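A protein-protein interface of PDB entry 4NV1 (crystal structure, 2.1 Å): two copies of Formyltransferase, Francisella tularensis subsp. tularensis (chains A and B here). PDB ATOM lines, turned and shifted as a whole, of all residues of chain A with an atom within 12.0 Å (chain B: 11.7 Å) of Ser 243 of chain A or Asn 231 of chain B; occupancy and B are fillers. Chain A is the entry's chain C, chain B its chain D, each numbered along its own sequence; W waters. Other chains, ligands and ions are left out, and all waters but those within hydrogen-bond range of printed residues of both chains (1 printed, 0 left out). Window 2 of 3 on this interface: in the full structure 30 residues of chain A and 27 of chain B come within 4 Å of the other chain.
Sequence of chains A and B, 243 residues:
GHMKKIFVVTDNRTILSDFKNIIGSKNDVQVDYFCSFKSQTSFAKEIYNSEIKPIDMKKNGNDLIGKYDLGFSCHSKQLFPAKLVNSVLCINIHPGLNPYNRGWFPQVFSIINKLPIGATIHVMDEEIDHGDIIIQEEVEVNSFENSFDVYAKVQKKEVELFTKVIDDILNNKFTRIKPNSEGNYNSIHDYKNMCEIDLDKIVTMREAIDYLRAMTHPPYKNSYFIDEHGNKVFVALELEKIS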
ATOM      1  N   GLU A 140     -10.069  -4.804   2.135  1.00  0.00           N
ATOM      2  CA  GLU A 140      -8.649  -4.817   2.553  1.00  0.00           C
ATOM      3  C   GLU A 140      -8.272  -6.208   3.075  1.00  0.00           C
ATOM      4  O   GLU A 140      -9.061  -6.860   3.791  1.00  0.00           O
ATOM      5  CB  GLU A 140      -8.431  -3.901   3.771  1.00  0.00           C
ATOM      6  CG  GLU A 140      -8.437  -2.408   3.487  1.00  0.00           C
ATOM      7  CD  GLU A 140      -7.797  -1.592   4.608  1.00  0.00           C
ATOM      8  OE1 GLU A 140      -8.197  -1.776   5.787  1.00  0.00           O
ATOM      9  OE2 GLU A 140      -6.905  -0.756   4.302  1.00  0.00           O
ATOM     10  N   VAL A 141      -7.087  -6.666   2.737  1.00  0.00           N
ATOM     11  CA  VAL A 141      -6.547  -7.853   3.384  1.00  0.00           C
ATOM     12  C   VAL A 141      -5.494  -7.373   4.373  1.00  0.00           C
ATOM     13  O   VAL A 141      -4.416  -6.905   3.968  1.00  0.00           O
ATOM     14  CB  VAL A 141      -5.893  -8.776   2.381  1.00  0.00           C
ATOM     15  CG1 VAL A 141      -5.331 -10.000   3.100  1.00  0.00           C
ATOM     16  CG2 VAL A 141      -6.870  -9.187   1.318  1.00  0.00           C
ATOM     17  N   ASN A 142      -5.796  -7.477   5.660  1.00  0.00           N
ATOM     18  CA  ASN A 142      -4.756  -7.190   6.658  1.00  0.00           C
ATOM     19  C   ASN A 142      -3.773  -8.320   6.987  1.00  0.00           C
ATOM     20  O   ASN A 142      -4.061  -9.518   6.765  1.00  0.00           O
ATOM     21  CB  ASN A 142      -5.473  -6.696   7.907  1.00  0.00           C
ATOM     22  CG  ASN A 142      -6.264  -5.426   7.643  1.00  0.00           C
ATOM     23  OD1 ASN A 142      -5.765  -4.510   7.012  1.00  0.00           O
ATOM     24  ND2 ASN A 142      -7.500  -5.380   8.103  1.00  0.00           N
ATOM     25  N   SER A 143      -2.623  -7.969   7.585  1.00  0.00           N
ATOM     26  CA  SER A 143      -1.535  -8.941   7.821  1.00  0.00           C
ATOM     27  C   SER A 143      -1.963 -10.124   8.686  1.00  0.00           C
ATOM     28  O   SER A 143      -1.447 -11.221   8.515  1.00  0.00           O
ATOM     29  CB  SER A 143      -0.351  -8.295   8.520  1.00  0.00           C
ATOM     30  OG  SER A 143      -0.795  -7.737   9.742  1.00  0.00           O
ATOM     31  N   PHE A 144      -2.918  -9.871   9.570  1.00  0.00           N
ATOM     32  CA  PHE A 144      -3.276 -10.776  10.615  1.00  0.00           C
ATOM     33  C   PHE A 144      -4.515 -11.633  10.289  1.00  0.00           C
ATOM     34  O   PHE A 144      -4.995 -12.354  11.140  1.00  0.00           O
ATOM     35  CB  PHE A 144      -3.481  -9.976  11.872  1.00  0.00           C
ATOM     36  CG  PHE A 144      -4.441  -8.832  11.734  1.00  0.00           C
ATOM     37  CD1 PHE A 144      -3.985  -7.534  11.497  1.00  0.00           C
ATOM     38  CD2 PHE A 144      -5.796  -9.007  12.008  1.00  0.00           C
ATOM     39  CE1 PHE A 144      -4.852  -6.469  11.436  1.00  0.00           C
ATOM     40  CE2 PHE A 144      -6.676  -7.932  11.954  1.00  0.00           C
ATOM     41  CZ  PHE A 144      -6.207  -6.662  11.649  1.00  0.00           C
ATOM     42  N   GLU A 145      -4.955 -11.643   9.042  1.00  0.00           N
ATOM     43  CA  GLU A 145      -6.188 -12.275   8.628  1.00  0.00           C
ATOM     44  C   GLU A 145      -5.886 -13.501   7.848  1.00  0.00           C
ATOM     45  O   GLU A 145      -4.876 -13.542   7.159  1.00  0.00           O
ATOM     46  CB  GLU A 145      -6.986 -11.357   7.677  1.00  0.00           C
ATOM     47  CG  GLU A 145      -7.404 -10.101   8.373  1.00  0.00           C
ATOM     48  CD  GLU A 145      -8.201  -9.084   7.571  1.00  0.00           C
ATOM     49  OE1 GLU A 145      -8.065  -9.080   6.339  1.00  0.00           O
ATOM     50  OE2 GLU A 145      -8.898  -8.268   8.247  1.00  0.00           O
ATOM     51  N   LYS A 153     -15.396 -10.699   5.808  1.00  0.00           N
ATOM     52  CA  LYS A 153     -15.516  -9.301   5.364  1.00  0.00           C
ATOM     53  C   LYS A 153     -16.207  -9.219   4.027  1.00  0.00           C
ATOM     54  O   LYS A 153     -16.962  -8.278   3.826  1.00  0.00           O
ATOM     55  CB  LYS A 153     -14.163  -8.564   5.211  1.00  0.00           C
ATOM     56  CG  LYS A 153     -13.773  -7.811   6.463  1.00  0.00           C
ATOM     57  CD  LYS A 153     -12.303  -7.961   6.839  1.00  0.00           C
ATOM     58  CE  LYS A 153     -11.422  -7.557   5.705  1.00  0.00           C
ATOM     59  NZ  LYS A 153     -10.271  -6.785   6.214  1.00  0.00           N
ATOM     60  N   ARG A 206       7.641 -14.286   4.552  1.00  0.00           N
ATOM     61  CA  ARG A 206       6.424 -13.555   4.188  1.00  0.00           C
ATOM     62  C   ARG A 206       5.476 -14.402   3.358  1.00  0.00           C
ATOM     63  O   ARG A 206       4.286 -14.489   3.618  1.00  0.00           O
ATOM     64  CB  ARG A 206       6.735 -12.317   3.360  1.00  0.00           C
ATOM     65  CG  ARG A 206       5.450 -11.751   2.800  1.00  0.00           C
ATOM     66  CD  ARG A 206       5.706 -10.403   2.175  1.00  0.00           C
ATOM     67  NE  ARG A 206       5.746  -9.341   3.159  1.00  0.00           N
ATOM     68  CZ  ARG A 206       6.819  -8.705   3.600  1.00  0.00           C
ATOM     69  NH1 ARG A 206       6.623  -7.740   4.479  1.00  0.00           N
ATOM     70  NH2 ARG A 206       8.057  -9.055   3.279  1.00  0.00           N
ATOM     71  N   ILE A 209       4.048 -17.517   5.234  1.00  0.00           N
ATOM     72  CA  ILE A 209       2.984 -17.046   6.074  1.00  0.00           C
ATOM     73  C   ILE A 209       1.720 -16.696   5.285  1.00  0.00           C
ATOM     74  O   ILE A 209       0.604 -17.069   5.697  1.00  0.00           O
ATOM     75  CB  ILE A 209       3.466 -15.905   6.959  1.00  0.00           C
ATOM     76  CG1 ILE A 209       4.342 -16.540   8.012  1.00  0.00           C
ATOM     77  CG2 ILE A 209       2.298 -15.143   7.569  1.00  0.00           C
ATOM     78  CD1 ILE A 209       5.179 -15.522   8.746  1.00  0.00           C
ATOM     79  N   ARG A 213      -1.730 -18.686   5.889  1.00  0.00           N
ATOM     80  CA  ARG A 213      -2.956 -18.002   6.194  1.00  0.00           C
ATOM     81  C   ARG A 213      -4.037 -18.054   5.114  1.00  0.00           C
ATOM     82  O   ARG A 213      -5.250 -18.162   5.442  1.00  0.00           O
ATOM     83  CB  ARG A 213      -2.728 -16.606   6.773  1.00  0.00           C
ATOM     84  CG  ARG A 213      -2.387 -15.527   5.737  1.00  0.00           C
ATOM     85  CD  ARG A 213      -1.716 -14.361   6.402  1.00  0.00           C
ATOM     86  NE  ARG A 213      -1.208 -13.324   5.508  1.00  0.00           N
ATOM     87  CZ  ARG A 213      -1.820 -12.162   5.292  1.00  0.00           C
ATOM     88  NH1 ARG A 213      -3.006 -11.932   5.784  1.00  0.00           N
ATOM     89  NH2 ARG A 213      -1.264 -11.223   4.518  1.00  0.00           N
ATOM     90  N   LEU A 239      -2.974 -16.392  13.897  1.00  0.00           N
ATOM     91  CA  LEU A 239      -2.342 -15.080  13.965  1.00  0.00           C
ATOM     92  C   LEU A 239      -3.097 -14.201  14.929  1.00  0.00           C
ATOM     93  O   LEU A 239      -4.320 -14.154  14.898  1.00  0.00           O
ATOM     94  CB  LEU A 239      -2.387 -14.390  12.609  1.00  0.00           C
ATOM     95  CG  LEU A 239      -1.710 -15.214  11.561  1.00  0.00           C
ATOM     96  CD1 LEU A 239      -2.613 -15.517  10.410  1.00  0.00           C
ATOM     97  CD2 LEU A 239      -0.480 -14.527  11.017  1.00  0.00           C
ATOM     98  N   GLU A 240      -2.368 -13.389  15.685  1.00  0.00           N
ATOM     99  CA  GLU A 240      -3.021 -12.524  16.644  1.00  0.00           C
ATOM    100  C   GLU A 240      -2.302 -11.213  16.723  1.00  0.00           C
ATOM    101  O   GLU A 240      -1.123 -11.129  17.077  1.00  0.00           O
ATOM    102  CB  GLU A 240      -3.149 -13.167  18.030  1.00  0.00           C
ATOM    103  CG  GLU A 240      -3.680 -12.204  19.089  1.00  0.00           C
ATOM    104  CD  GLU A 240      -4.111 -12.876  20.394  1.00  0.00           C
ATOM    105  OE1 GLU A 240      -4.985 -12.284  21.069  1.00  0.00           O
ATOM    106  OE2 GLU A 240      -3.601 -13.976  20.736  1.00  0.00           O
ATOM    107  N   LYS A 241      -3.071 -10.169  16.448  1.00  0.00           N
ATOM    108  CA  LYS A 241      -2.540  -8.825  16.559  1.00  0.00           C
ATOM    109  C   LYS A 241      -2.575  -8.501  18.055  1.00  0.00           C
ATOM    110  O   LYS A 241      -3.570  -8.657  18.764  1.00  0.00           O
ATOM    111  CB  LYS A 241      -3.351  -7.835  15.720  1.00  0.00           C
ATOM    112  CG  LYS A 241      -2.638  -6.509  15.544  1.00  0.00           C
ATOM    113  CD  LYS A 241      -3.590  -5.306  15.520  1.00  0.00           C
ATOM    114  CE  LYS A 241      -4.671  -5.399  14.455  1.00  0.00           C
ATOM    115  NZ  LYS A 241      -6.055  -5.174  14.966  1.00  0.00           N
ATOM    116  N   ILE A 242      -1.400  -8.145  18.525  1.00  0.00           N
ATOM    117  CA  ILE A 242      -1.249  -7.528  19.797  1.00  0.00           C
ATOM    118  C   ILE A 242      -0.923  -6.089  19.437  1.00  0.00           C
ATOM    119  O   ILE A 242       0.248  -5.762  19.209  1.00  0.00           O
ATOM    120  CB  ILE A 242      -0.095  -8.193  20.535  1.00  0.00           C
ATOM    121  CG1 ILE A 242      -0.547  -9.603  20.927  1.00  0.00           C
ATOM    122  CG2 ILE A 242       0.366  -7.309  21.694  1.00  0.00           C
ATOM    123  CD1 ILE A 242      -1.866  -9.658  21.681  1.00  0.00           C
ATOM    124  N   SER A 243      -1.973  -5.273  19.318  1.00  0.00           N
ATOM    125  CA  SER A 243      -1.854  -3.810  19.346  1.00  0.00           C
ATOM    126  C   SER A 243      -3.155  -3.215  19.890  1.00  0.00           C
ATOM    127  O   SER A 243      -3.873  -3.888  20.636  1.00  0.00           O
ATOM    128  CB  SER A 243      -1.488  -3.243  17.966  1.00  0.00           C
ATOM    129  OG  SER A 243      -0.211  -3.694  17.532  1.00  0.00           O
ATOM    130  OXT SER A 243      -3.521  -2.069  19.622  1.00  0.00           O
ATOM    131  N   CYS B 195      12.732 -15.107  18.126  1.00  0.00           N
ATOM    132  CA  CYS B 195      11.308 -14.828  18.199  1.00  0.00           C
ATOM    133  C   CYS B 195      10.803 -13.730  17.234  1.00  0.00           C
ATOM    134  O   CYS B 195       9.636 -13.790  16.793  1.00  0.00           O
ATOM    135  CB  CYS B 195      10.864 -14.599  19.654  1.00  0.00           C
ATOM    136  SG  CYS B 195      10.891 -16.096  20.687  1.00  0.00           S
ATOM    137  N   GLU B 196      11.664 -12.805  16.807  1.00  0.00           N
ATOM    138  CA  GLU B 196      11.210 -11.808  15.830  1.00  0.00           C
ATOM    139  C   GLU B 196      11.399 -12.393  14.445  1.00  0.00           C
ATOM    140  O   GLU B 196      12.496 -12.776  14.029  1.00  0.00           O
ATOM    141  CB  GLU B 196      11.893 -10.444  15.987  1.00  0.00           C
ATOM    142  CG  GLU B 196      11.715  -9.487  14.803  1.00  0.00           C
ATOM    143  CD  GLU B 196      12.511  -8.185  14.978  1.00  0.00           C
ATOM    144  OE1 GLU B 196      13.743  -8.243  14.842  1.00  0.00           O
ATOM    145  OE2 GLU B 196      11.936  -7.119  15.293  1.00  0.00           O
ATOM    146  N   ILE B 197      10.290 -12.455  13.713  1.00  0.00           N
ATOM    147  CA  ILE B 197      10.343 -13.035  12.394  1.00  0.00           C
ATOM    148  C   ILE B 197      10.985 -12.033  11.434  1.00  0.00           C
ATOM    149  O   ILE B 197      10.722 -10.839  11.548  1.00  0.00           O
ATOM    150  CB  ILE B 197       8.910 -13.370  11.972  1.00  0.00           C
ATOM    151  CG1 ILE B 197       8.474 -14.668  12.646  1.00  0.00           C
ATOM    152  CG2 ILE B 197       8.808 -13.513  10.473  1.00  0.00           C
ATOM    153  CD1 ILE B 197       7.002 -14.936  12.492  1.00  0.00           C
ATOM    154  N   LEU B 199      10.439 -11.187   7.948  1.00  0.00           N
ATOM    155  CA  LEU B 199       9.584 -11.461   6.764  1.00  0.00           C
ATOM    156  C   LEU B 199      10.355 -11.663   5.467  1.00  0.00           C
ATOM    157  O   LEU B 199       9.948 -12.474   4.633  1.00  0.00           O
ATOM    158  CB  LEU B 199       8.512 -10.387   6.651  1.00  0.00           C
ATOM    159  CG  LEU B 199       7.616 -10.277   7.902  1.00  0.00           C
ATOM    160  CD1 LEU B 199       6.922  -8.926   8.113  1.00  0.00           C
ATOM    161  CD2 LEU B 199       6.627 -11.423   7.940  1.00  0.00           C
ATOM    162  N   LYS B 221       2.646 -16.947  23.786  1.00  0.00           N
ATOM    163  CA  LYS B 221       2.725 -16.305  22.514  1.00  0.00           C
ATOM    164  C   LYS B 221       4.199 -15.972  22.322  1.00  0.00           C
ATOM    165  O   LYS B 221       4.735 -15.152  23.076  1.00  0.00           O
ATOM    166  CB  LYS B 221       1.864 -15.030  22.563  1.00  0.00           C
ATOM    167  CG  LYS B 221       0.399 -15.242  22.941  1.00  0.00           C
ATOM    168  CD  LYS B 221      -0.248 -13.909  23.317  1.00  0.00           C
ATOM    169  CE  LYS B 221      -1.409 -14.050  24.298  1.00  0.00           C
ATOM    170  NZ  LYS B 221      -1.234 -13.138  25.471  1.00  0.00           N
ATOM    171  N   SER B 223       6.467 -16.414  18.674  1.00  0.00           N
ATOM    172  CA  SER B 223       6.993 -15.793  17.449  1.00  0.00           C
ATOM    173  C   SER B 223       6.068 -14.663  16.979  1.00  0.00           C
ATOM    174  O   SER B 223       4.840 -14.720  17.218  1.00  0.00           O
ATOM    175  CB  SER B 223       7.245 -16.824  16.354  1.00  0.00           C
ATOM    176  OG  SER B 223       6.060 -17.437  15.890  1.00  0.00           O
ATOM    177  N   TYR B 224       6.620 -13.616  16.356  1.00  0.00           N
ATOM    178  CA  TYR B 224       5.785 -12.497  15.883  1.00  0.00           C
ATOM    179  C   TYR B 224       6.533 -11.765  14.784  1.00  0.00           C
ATOM    180  O   TYR B 224       7.745 -11.907  14.664  1.00  0.00           O
ATOM    181  CB  TYR B 224       5.392 -11.542  17.024  1.00  0.00           C
ATOM    182  CG  TYR B 224       6.631 -10.874  17.550  1.00  0.00           C
ATOM    183  CD1 TYR B 224       7.387 -11.466  18.571  1.00  0.00           C
ATOM    184  CD2 TYR B 224       7.172  -9.778  16.879  1.00  0.00           C
ATOM    185  CE1 TYR B 224       8.581 -10.902  18.979  1.00  0.00           C
ATOM    186  CE2 TYR B 224       8.380  -9.224  17.262  1.00  0.00           C
ATOM    187  CZ  TYR B 224       9.077  -9.813  18.294  1.00  0.00           C
ATOM    188  OH  TYR B 224      10.230  -9.244  18.698  1.00  0.00           O
ATOM    189  N   PHE B 225       5.769 -11.083  13.927  1.00  0.00           N
ATOM    190  CA  PHE B 225       6.316 -10.217  12.880  1.00  0.00           C
ATOM    191  C   PHE B 225       5.768  -8.813  13.147  1.00  0.00           C
ATOM    192  O   PHE B 225       4.845  -8.640  13.913  1.00  0.00           O
ATOM    193  CB  PHE B 225       6.057 -10.762  11.471  1.00  0.00           C
ATOM    194  CG  PHE B 225       4.600 -10.891  11.113  1.00  0.00           C
ATOM    195  CD1 PHE B 225       3.930 -12.088  11.337  1.00  0.00           C
ATOM    196  CD2 PHE B 225       3.895  -9.835  10.577  1.00  0.00           C
ATOM    197  CE1 PHE B 225       2.604 -12.212  11.009  1.00  0.00           C
ATOM    198  CE2 PHE B 225       2.554  -9.968  10.256  1.00  0.00           C
ATOM    199  CZ  PHE B 225       1.907 -11.152  10.438  1.00  0.00           C
ATOM    200  N   ILE B 226       6.456  -7.786  12.669  1.00  0.00           N
ATOM    201  CA  ILE B 226       5.921  -6.429  12.741  1.00  0.00           C
ATOM    202  C   ILE B 226       5.494  -6.176  11.310  1.00  0.00           C
ATOM    203  O   ILE B 226       6.282  -6.342  10.377  1.00  0.00           O
ATOM    204  CB  ILE B 226       6.931  -5.347  13.181  1.00  0.00           C
ATOM    205  CG1 ILE B 226       7.296  -5.461  14.657  1.00  0.00           C
ATOM    206  CG2 ILE B 226       6.261  -3.985  13.109  1.00  0.00           C
ATOM    207  CD1 ILE B 226       8.262  -6.576  14.925  1.00  0.00           C
ATOM    208  N   ASP B 227       4.233  -5.812  11.124  1.00  0.00           N
ATOM    209  CA  ASP B 227       3.771  -5.623   9.757  1.00  0.00           C
ATOM    210  C   ASP B 227       4.005  -4.154   9.355  1.00  0.00           C
ATOM    211  O   ASP B 227       4.538  -3.363  10.143  1.00  0.00           O
ATOM    212  CB  ASP B 227       2.295  -6.023   9.651  1.00  0.00           C
ATOM    213  CG  ASP B 227       1.359  -5.002  10.240  1.00  0.00           C
ATOM    214  OD1 ASP B 227       1.823  -3.874  10.538  1.00  0.00           O
ATOM    215  OD2 ASP B 227       0.149  -5.317  10.365  1.00  0.00           O
ATOM    216  N   GLU B 228       3.539  -3.797   8.161  1.00  0.00           N
ATOM    217  CA  GLU B 228       3.792  -2.485   7.564  1.00  0.00           C
ATOM    218  C   GLU B 228       3.172  -1.321   8.343  1.00  0.00           C
ATOM    219  O   GLU B 228       3.597  -0.190   8.224  1.00  0.00           O
ATOM    220  CB  GLU B 228       3.343  -2.479   6.098  1.00  0.00           C
ATOM    221  CG  GLU B 228       1.826  -2.511   5.886  1.00  0.00           C
ATOM    222  CD  GLU B 228       1.399  -2.580   4.420  1.00  0.00           C
ATOM    223  OE1 GLU B 228       0.305  -3.115   4.117  1.00  0.00           O
ATOM    224  OE2 GLU B 228       2.163  -2.121   3.546  1.00  0.00           O
ATOM    225  N   HIS B 229       2.206  -1.569   9.202  1.00  0.00           N
ATOM    226  CA  HIS B 229       1.693  -0.491  10.024  1.00  0.00           C
ATOM    227  C   HIS B 229       2.278  -0.575  11.422  1.00  0.00           C
ATOM    228  O   HIS B 229       1.802   0.078  12.362  1.00  0.00           O
ATOM    229  CB  HIS B 229       0.156  -0.562  10.013  1.00  0.00           C
ATOM    230  CG  HIS B 229      -0.427  -0.830   8.648  1.00  0.00           C
ATOM    231  ND1 HIS B 229      -0.679   0.168   7.730  1.00  0.00           N
ATOM    232  CD2 HIS B 229      -0.779  -1.990   8.041  1.00  0.00           C
ATOM    233  CE1 HIS B 229      -1.157  -0.363   6.620  1.00  0.00           C
ATOM    234  NE2 HIS B 229      -1.241  -1.670   6.788  1.00  0.00           N
ATOM    235  N   GLY B 230       3.316  -1.403  11.549  1.00  0.00           N
ATOM    236  CA  GLY B 230       3.880  -1.788  12.838  1.00  0.00           C
ATOM    237  C   GLY B 230       2.878  -2.304  13.836  1.00  0.00           C
ATOM    238  O   GLY B 230       2.947  -1.932  15.007  1.00  0.00           O
ATOM    239  N   ASN B 231       1.905  -3.103  13.399  1.00  0.00           N
ATOM    240  CA  ASN B 231       1.165  -3.921  14.378  1.00  0.00           C
ATOM    241  C   ASN B 231       2.132  -5.086  14.660  1.00  0.00           C
ATOM    242  O   ASN B 231       2.820  -5.589  13.764  1.00  0.00           O
ATOM    243  CB  ASN B 231      -0.209  -4.481  13.915  1.00  0.00           C
ATOM    244  CG  ASN B 231      -1.151  -3.435  13.292  1.00  0.00           C
ATOM    245  OD1 ASN B 231      -1.624  -2.534  13.965  1.00  0.00           O
ATOM    246  ND2 ASN B 231      -1.461  -3.588  12.017  1.00  0.00           N
ATOM    247  N   LYS B 232       2.207  -5.486  15.917  1.00  0.00           N
ATOM    248  CA  LYS B 232       2.971  -6.677  16.277  1.00  0.00           C
ATOM    249  C   LYS B 232       2.013  -7.864  16.207  1.00  0.00           C
ATOM    250  O   LYS B 232       1.011  -7.880  16.954  1.00  0.00           O
ATOM    251  CB  LYS B 232       3.536  -6.522  17.685  1.00  0.00           C
ATOM    252  CG  LYS B 232       4.539  -7.595  18.066  1.00  0.00           C
ATOM    253  CD  LYS B 232       5.540  -7.089  19.095  1.00  0.00           C
ATOM    254  CE  LYS B 232       6.133  -8.194  19.961  1.00  0.00           C
ATOM    255  NZ  LYS B 232       6.059  -7.825  21.402  1.00  0.00           N
ATOM    256  N   VAL B 233       2.289  -8.800  15.292  1.00  0.00           N
ATOM    257  CA  VAL B 233       1.400  -9.937  15.064  1.00  0.00           C
ATOM    258  C   VAL B 233       1.992 -11.289  15.507  1.00  0.00           C
ATOM    259  O   VAL B 233       2.908 -11.771  14.900  1.00  0.00           O
ATOM    260  CB  VAL B 233       1.005 -10.034  13.579  1.00  0.00           C
ATOM    261  CG1 VAL B 233      -0.063 -11.126  13.422  1.00  0.00           C
ATOM    262  CG2 VAL B 233       0.507  -8.671  13.062  1.00  0.00           C
ATOM    263  N   PHE B 234       1.450 -11.929  16.540  1.00  0.00           N
ATOM    264  CA  PHE B 234       1.947 -13.242  17.012  1.00  0.00           C
ATOM    265  C   PHE B 234       1.442 -14.379  16.136  1.00  0.00           C
ATOM    266  O   PHE B 234       0.335 -14.344  15.633  1.00  0.00           O
ATOM    267  CB  PHE B 234       1.614 -13.446  18.488  1.00  0.00           C
ATOM    268  CG  PHE B 234       2.515 -12.685  19.423  1.00  0.00           C
ATOM    269  CD1 PHE B 234       3.648 -13.258  19.944  1.00  0.00           C
ATOM    270  CD2 PHE B 234       2.242 -11.369  19.760  1.00  0.00           C
ATOM    271  CE1 PHE B 234       4.508 -12.545  20.755  1.00  0.00           C
ATOM    272  CE2 PHE B 234       3.075 -10.642  20.608  1.00  0.00           C
ATOM    273  CZ  PHE B 234       4.234 -11.232  21.097  1.00  0.00           C
ATOM    274  N   VAL B 235       2.289 -15.314  15.786  1.00  0.00           N
ATOM    275  CA  VAL B 235       1.865 -16.383  14.886  1.00  0.00           C
ATOM    276  C   VAL B 235       2.157 -17.728  15.586  1.00  0.00           C
ATOM    277  O   VAL B 235       3.148 -17.876  16.308  1.00  0.00           O
ATOM    278  CB  VAL B 235       2.514 -16.323  13.493  1.00  0.00           C
ATOM    279  CG1 VAL B 235       2.536 -14.884  12.983  1.00  0.00           C
ATOM    280  CG2 VAL B 235       3.934 -16.780  13.530  1.00  0.00           C
HETATM  281  O   HOH W   1      -2.134  -5.146   8.190  1.00  0.00           O
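The side-chain hydroxyl (OG) of Ser 143 of chain A is in hydrogen-bond range of the side-chain carboxylate (OD2) of Asp 227 of chain B.
The backbone NH (N) of Arg 206 of chain A is in hydrogen-bond range of the backbone carbonyl oxygen (O) of Leu 199 of chain B, at 2.9 Å.
The backbone carbonyl oxygen of Glu 240 of chain A lies within hydrogen-bond range of the backbone NH of Phe 234 of chain B.
N of Lys 232 of chain B lies within hydrogen-bond range of OG of Ser 243 of chain A (3.4 Å).
O of Lys 232 of chain B lies within hydrogen-bond range of N of Ile 242 of chain A (2.9 Å).
The side-chain carboxylate (OD1) of Asp 227 of chain B is in hydrogen-bond range of the backbone NH (N) of Gly 230 of chain B (3.1 Å).
The backbone carbonyl oxygen of Ser 143 of chain A lies within hydrogen-bond range of the guanidinium group of Arg 213 of chain A (3.2 Å).
O of Phe 225 of chain B sits at hydrogen-bond distance from N of Val 233 of chain B, 2.9 Å away.
The backbone carbonyl oxygen (O) of Val 235 of chain B is in hydrogen-bond range of the side-chain hydroxyl (OG) of Ser 223 of chain B, 3.0 Å away.
The side-chain carboxylate (OD2) of Asp 227 of chain B lies within hydrogen-bond range of the side-chain amide nitrogen (ND2) of Asn 231 of chain B (2.9 Å).
OD1 of Asp 227 of chain B is in hydrogen-bond range of N of His 229 of chain B.
Among the printed residues, pairs that only touch across the chains: Leu 239 of chain A with Phe 234 of chain B, Glu 240 of chain A with Val 233 of chain B, Ser 243 of chain A with Asn 231 of chain B, Ile 242 of chain A with Phe 234 of chain B, Lys 241 of chain A with Asn 231 of chain B, Leu 239 of chain A with Val 235 of chain B, Ser 143 of chain A with Val 233 of chain B, Lys 241 of chain A with Lys 232 of chain B, Ser 143 of chain A with Phe 225 of chain B, Leu 239 of chain A with Phe 225 of chain B, Glu 240 of chain A with Lys 232 of chain B and Phe 144 of chain A with Val 233 of chain B.
Printed residues of chain A within 4 Å of Asn 231 of chain B: Lys 241 (3.6 Å) and Ser 243 (3.4 Å).
Of the printed residues of chain B, Lys 241 of chain A touches Asn 231 and Lys 232.
Of the printed residues of chain A, Phe 225 of chain B touches Ser 143 and Leu 239.
No residue of chain A comes within 4 Å of Ile 226 of chain B.
Of chain A, only Ser 143 (2.7 Å) comes within 4 Å of Asp 227 of chain B.
No residue of chain A comes within 4 Å of His 229 of chain B.
Gly 230 of chain B touches none of the printed residues of chain A.
Of the printed residues of chain A, Val 233 of chain B touches Ser 143 (3.7 Å), Phe 144 (3.9 Å) and Glu 240 (3.4 Å).
Of the printed residues of chain A, Leu 199 of chain B touches Arg 206 (2.9 Å).
Of the printed residues of chain B, Phe 144 of chain A touches Val 233.
Printed residues of chain B within 4 Å of Ser 143 of chain A: Phe 225 (3.8 Å), Asp 227 (2.7 Å) and Val 233 (3.7 Å).
Of the printed residues of chain B, Arg 206 of chain A touches Leu 199.
Of the printed residues of chain B, Leu 239 of chain A touches Phe 225 (3.9 Å), Phe 234 (3.2 Å) and Val 235 (3.6 Å).
Ile 197 of chain B touches none of the printed residues of chain A.
The nearest residue of chain A that does not touch Asn 231 of chain B is Phe 144 of chain A (4.5 Å).
The nearest printed residue of chain B that does not touch Leu 239 of chain A is Val 233 of chain B (4.1 Å).
Of the 15 printed residues of chain A, 8 touch a printed residue of chain B.
Hydrophobic or aromatic side chains of chain A that line the printed part of chain B: Phe 144, Leu 239 and Ile 242.
Printed residues of chain B that touch a printed residue of chain A: Leu 199, Phe 225, Asp 227, Asn 231, Lys 232, Val 233, Phe 234 and Val 235.
Among the printed residues, no Asp or Glu carboxylate lies within 4 Å of a Lys or Arg side-chain nitrogen of the other chain.
No position is printed for both chains.
Water W1 lies within hydrogen-bond range of the backbone NH (N) of Ser 143 of chain A and the side-chain carboxylate (OD2) of Asp 227 of chain B.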
